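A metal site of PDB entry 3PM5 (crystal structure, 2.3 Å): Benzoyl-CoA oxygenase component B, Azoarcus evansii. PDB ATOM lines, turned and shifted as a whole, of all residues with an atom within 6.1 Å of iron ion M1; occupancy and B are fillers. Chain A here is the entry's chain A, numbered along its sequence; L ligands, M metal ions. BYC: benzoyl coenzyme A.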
ATOM      1  N   GLU A 120     -18.073   1.179   2.419  1.00  0.00           N
ATOM      2  CA  GLU A 120     -17.477   1.237   3.750  1.00  0.00           C
ATOM      3  C   GLU A 120     -15.956   1.051   3.688  1.00  0.00           C
ATOM      4  O   GLU A 120     -15.248   1.986   4.037  1.00  0.00           O
ATOM      5  CB  GLU A 120     -18.129   0.219   4.695  1.00  0.00           C
ATOM      6  CG  GLU A 120     -19.664   0.269   4.766  1.00  0.00           C
ATOM      7  CD  GLU A 120     -20.225   1.543   5.347  1.00  0.00           C
ATOM      8  OE1 GLU A 120     -19.411   2.297   6.001  1.00  0.00           O
ATOM      9  OE2 GLU A 120     -21.463   1.811   5.153  1.00  0.00           O
ATOM     10  N   VAL A 146     -14.051   7.369  12.804  1.00  0.00           N
ATOM     11  CA  VAL A 146     -14.884   7.282  11.656  1.00  0.00           C
ATOM     12  C   VAL A 146     -14.398   6.061  10.944  1.00  0.00           C
ATOM     13  O   VAL A 146     -15.199   5.235  10.556  1.00  0.00           O
ATOM     14  CB  VAL A 146     -14.801   8.624  10.798  1.00  0.00           C
ATOM     15  CG1 VAL A 146     -15.292   8.456   9.405  1.00  0.00           C
ATOM     16  CG2 VAL A 146     -15.543   9.812  11.470  1.00  0.00           C
ATOM     17  N   GLU A 150     -16.569   2.772  10.048  1.00  0.00           N
ATOM     18  CA  GLU A 150     -16.663   2.385   8.625  1.00  0.00           C
ATOM     19  C   GLU A 150     -16.418   0.873   8.578  1.00  0.00           C
ATOM     20  O   GLU A 150     -17.209   0.106   7.995  1.00  0.00           O
ATOM     21  CB  GLU A 150     -15.636   3.168   7.728  1.00  0.00           C
ATOM     22  CG  GLU A 150     -15.981   4.701   7.529  1.00  0.00           C
ATOM     23  CD  GLU A 150     -14.853   5.672   6.934  1.00  0.00           C
ATOM     24  OE1 GLU A 150     -13.625   5.492   7.073  1.00  0.00           O
ATOM     25  OE2 GLU A 150     -15.235   6.688   6.311  1.00  0.00           O
ATOM     26  N   HIS A 153     -19.205  -1.207   9.812  1.00  0.00           N
ATOM     27  CA  HIS A 153     -20.293  -1.230   8.853  1.00  0.00           C
ATOM     28  C   HIS A 153     -20.049  -2.218   7.740  1.00  0.00           C
ATOM     29  O   HIS A 153     -20.987  -2.830   7.258  1.00  0.00           O
ATOM     30  CB  HIS A 153     -20.495   0.177   8.332  1.00  0.00           C
ATOM     31  CG  HIS A 153     -21.066   1.082   9.366  1.00  0.00           C
ATOM     32  ND1 HIS A 153     -21.418   2.380   9.098  1.00  0.00           N
ATOM     33  CD2 HIS A 153     -21.409   0.847  10.652  1.00  0.00           C
ATOM     34  CE1 HIS A 153     -21.965   2.914  10.177  1.00  0.00           C
ATOM     35  NE2 HIS A 153     -21.959   2.002  11.134  1.00  0.00           N
ATOM     36  N   THR A 207     -17.494  13.919   5.044  1.00  0.00           N
ATOM     37  CA  THR A 207     -18.330  13.482   6.171  1.00  0.00           C
ATOM     38  C   THR A 207     -19.566  14.328   6.392  1.00  0.00           C
ATOM     39  O   THR A 207     -20.559  13.866   6.974  1.00  0.00           O
ATOM     40  CB  THR A 207     -17.554  13.323   7.447  1.00  0.00           C
ATOM     41  OG1 THR A 207     -16.810  14.514   7.698  1.00  0.00           O
ATOM     42  CG2 THR A 207     -16.594  12.140   7.293  1.00  0.00           C
ATOM     43  N   ASP A 211     -21.212  11.049   3.733  1.00  0.00           N
ATOM     44  CA  ASP A 211     -21.813  10.252   4.849  1.00  0.00           C
ATOM     45  C   ASP A 211     -23.302  10.489   4.978  1.00  0.00           C
ATOM     46  O   ASP A 211     -24.019   9.612   5.456  1.00  0.00           O
ATOM     47  CB  ASP A 211     -21.188  10.510   6.237  1.00  0.00           C
ATOM     48  CG  ASP A 211     -19.830   9.861   6.401  1.00  0.00           C
ATOM     49  OD1 ASP A 211     -19.000  10.042   5.515  1.00  0.00           O
ATOM     50  OD2 ASP A 211     -19.538   9.185   7.415  1.00  0.00           O
ATOM     51  N   GLU A 240     -23.715   6.612  12.659  1.00  0.00           N
ATOM     52  CA  GLU A 240     -23.460   7.633  11.617  1.00  0.00           C
ATOM     53  C   GLU A 240     -23.713   9.103  12.062  1.00  0.00           C
ATOM     54  O   GLU A 240     -23.122  10.014  11.497  1.00  0.00           O
ATOM     55  CB  GLU A 240     -24.246   7.312  10.334  1.00  0.00           C
ATOM     56  CG  GLU A 240     -23.735   7.992   9.072  1.00  0.00           C
ATOM     57  CD  GLU A 240     -22.512   7.269   8.437  1.00  0.00           C
ATOM     58  OE1 GLU A 240     -22.634   6.516   7.408  1.00  0.00           O
ATOM     59  OE2 GLU A 240     -21.404   7.482   8.960  1.00  0.00           O
ATOM     60  N   HIS A 243     -20.626  10.804  12.720  1.00  0.00           N
ATOM     61  CA  HIS A 243     -19.835  11.089  11.528  1.00  0.00           C
ATOM     62  C   HIS A 243     -20.277  12.406  10.924  1.00  0.00           C
ATOM     63  O   HIS A 243     -19.442  13.196  10.567  1.00  0.00           O
ATOM     64  CB  HIS A 243     -19.889   9.958  10.505  1.00  0.00           C
ATOM     65  CG  HIS A 243     -19.462   8.635  11.067  1.00  0.00           C
ATOM     66  ND1 HIS A 243     -19.266   7.526  10.294  1.00  0.00           N
ATOM     67  CD2 HIS A 243     -19.121   8.268  12.329  1.00  0.00           C
ATOM     68  CE1 HIS A 243     -18.881   6.519  11.048  1.00  0.00           C
ATOM     69  NE2 HIS A 243     -18.768   6.946  12.294  1.00  0.00           N
HETATM   70  N1A BYC L   1     -24.732   4.751 -13.531  1.00  0.00           N
HETATM   71  O1A BYC L   1     -32.120   3.647  -9.861  1.00  0.00           O
HETATM   72  P1A BYC L   1     -30.952   3.811 -10.875  1.00  0.00           P
HETATM   73  C1B BYC L   1     -22.567   5.312   2.638  1.00  0.00           C
HETATM   74  C1D BYC L   1     -29.629   3.585 -15.647  1.00  0.00           C
HETATM   75  S1P BYC L   1     -23.097   5.952   1.032  1.00  0.00           S
HETATM   76  C2A BYC L   1     -25.835   4.139 -12.847  1.00  0.00           C
HETATM   77  O2A BYC L   1     -30.414   5.202 -11.176  1.00  0.00           O
HETATM   78  P2A BYC L   1     -29.901   1.708  -9.445  1.00  0.00           P
HETATM   79  C2B BYC L   1     -21.219   5.772   3.055  1.00  0.00           C
HETATM   80  C2D BYC L   1     -29.762   2.285 -14.870  1.00  0.00           C
HETATM   81  O2D BYC L   1     -29.050   1.164 -15.308  1.00  0.00           O
HETATM   82  C2P BYC L   1     -24.618   5.069   0.511  1.00  0.00           C
HETATM   83  N3A BYC L   1     -27.080   3.876 -13.544  1.00  0.00           N
HETATM   84  O3A BYC L   1     -29.707   2.891 -10.478  1.00  0.00           O
HETATM   85  C3B BYC L   1     -20.858   7.164   2.772  1.00  0.00           C
HETATM   86  C3D BYC L   1     -31.211   2.136 -14.948  1.00  0.00           C
HETATM   87  O3D BYC L   1     -31.527   1.861 -16.317  1.00  0.00           O
HETATM   88  P3D BYC L   1     -32.962   1.363 -16.803  1.00  0.00           P
HETATM   89  C3P BYC L   1     -24.341   3.735  -0.123  1.00  0.00           C
HETATM   90  C4A BYC L   1     -27.233   4.265 -14.942  1.00  0.00           C
HETATM   91  O4A BYC L   1     -31.125   0.829  -9.734  1.00  0.00           O
HETATM   92  C4B BYC L   1     -19.535   7.645   3.199  1.00  0.00           C
HETATM   93  C4D BYC L   1     -31.654   3.510 -14.593  1.00  0.00           C
HETATM   94  O4D BYC L   1     -30.619   4.408 -15.009  1.00  0.00           O
HETATM   95  N4P BYC L   1     -25.582   3.005   0.010  1.00  0.00           N
HETATM   96  O57 BYC L   1     -23.024   4.309   3.115  1.00  0.00           O
HETATM   97  O5A BYC L   1     -28.629   0.890  -9.511  1.00  0.00           O
HETATM   98  C5B BYC L   1     -18.576   6.744   3.889  1.00  0.00           C
HETATM   99  C5D BYC L   1     -32.085   3.926 -13.204  1.00  0.00           C
HETATM  100  O5D BYC L   1     -31.335   3.196 -12.274  1.00  0.00           O
HETATM  101  C5M BYC L   1     -26.171   4.887 -15.618  1.00  0.00           C
HETATM  102  C5P BYC L   1     -26.372   2.722  -1.120  1.00  0.00           C
HETATM  103  O5P BYC L   1     -25.999   3.073  -2.234  1.00  0.00           O
HETATM  104  C6A BYC L   1     -24.886   5.138 -14.899  1.00  0.00           C
HETATM  105  N6A BYC L   1     -23.846   5.760 -15.597  1.00  0.00           N
HETATM  106  O6A BYC L   1     -30.099   2.410  -7.988  1.00  0.00           O
HETATM  107  C6B BYC L   1     -18.954   5.343   4.150  1.00  0.00           C
HETATM  108  C6P BYC L   1     -27.718   2.006  -0.852  1.00  0.00           C
HETATM  109  N7A BYC L   1     -26.555   5.149 -16.880  1.00  0.00           N
HETATM  110  O7A BYC L   1     -33.102  -0.079 -16.368  1.00  0.00           O
HETATM  111  C7B BYC L   1     -20.287   4.856   3.742  1.00  0.00           C
HETATM  112  C7P BYC L   1     -28.142   0.910  -1.757  1.00  0.00           C
HETATM  113  C8A BYC L   1     -27.842   4.714 -17.040  1.00  0.00           C
HETATM  114  O8A BYC L   1     -33.034   1.513 -18.294  1.00  0.00           O
HETATM  115  N8P BYC L   1     -28.181   1.284  -3.149  1.00  0.00           N
HETATM  116  N9A BYC L   1     -28.252   4.153 -15.844  1.00  0.00           N
HETATM  117  O9A BYC L   1     -34.073   2.184 -16.112  1.00  0.00           O
HETATM  118  C9P BYC L   1     -29.360   1.595  -3.899  1.00  0.00           C
HETATM  119  O9P BYC L   1     -30.510   1.566  -3.426  1.00  0.00           O
HETATM  120  CAP BYC L   1     -29.025   1.911  -5.320  1.00  0.00           C
HETATM  121  OAP BYC L   1     -27.664   1.702  -5.394  1.00  0.00           O
HETATM  122  CBP BYC L   1     -29.287   3.341  -5.833  1.00  0.00           C
HETATM  123  CCP BYC L   1     -29.146   3.318  -7.403  1.00  0.00           C
HETATM  124  CDP BYC L   1     -30.639   3.835  -5.455  1.00  0.00           C
HETATM  125  CEP BYC L   1     -28.232   4.274  -5.260  1.00  0.00           C
HETATM  126 FE    FE M   1     -19.798   7.305   8.080  1.00  0.00          FE
HETATM  127 FE    FE M   2     -20.983   3.873   7.200  1.00  0.00          FE
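Iron ion M1 is bound by the side-chain carboxylate of Glu 240 (1.8 Å), the side-chain carboxylate of Asp 211 (2.0 Å) and a ring nitrogen (ND1) of His 243 (2.3 Å).
Iron ion M1 has three donor atoms within binding distance.
The nearest printed residue that does not touch iron ion M1 is Glu 150 (4.7 Å).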
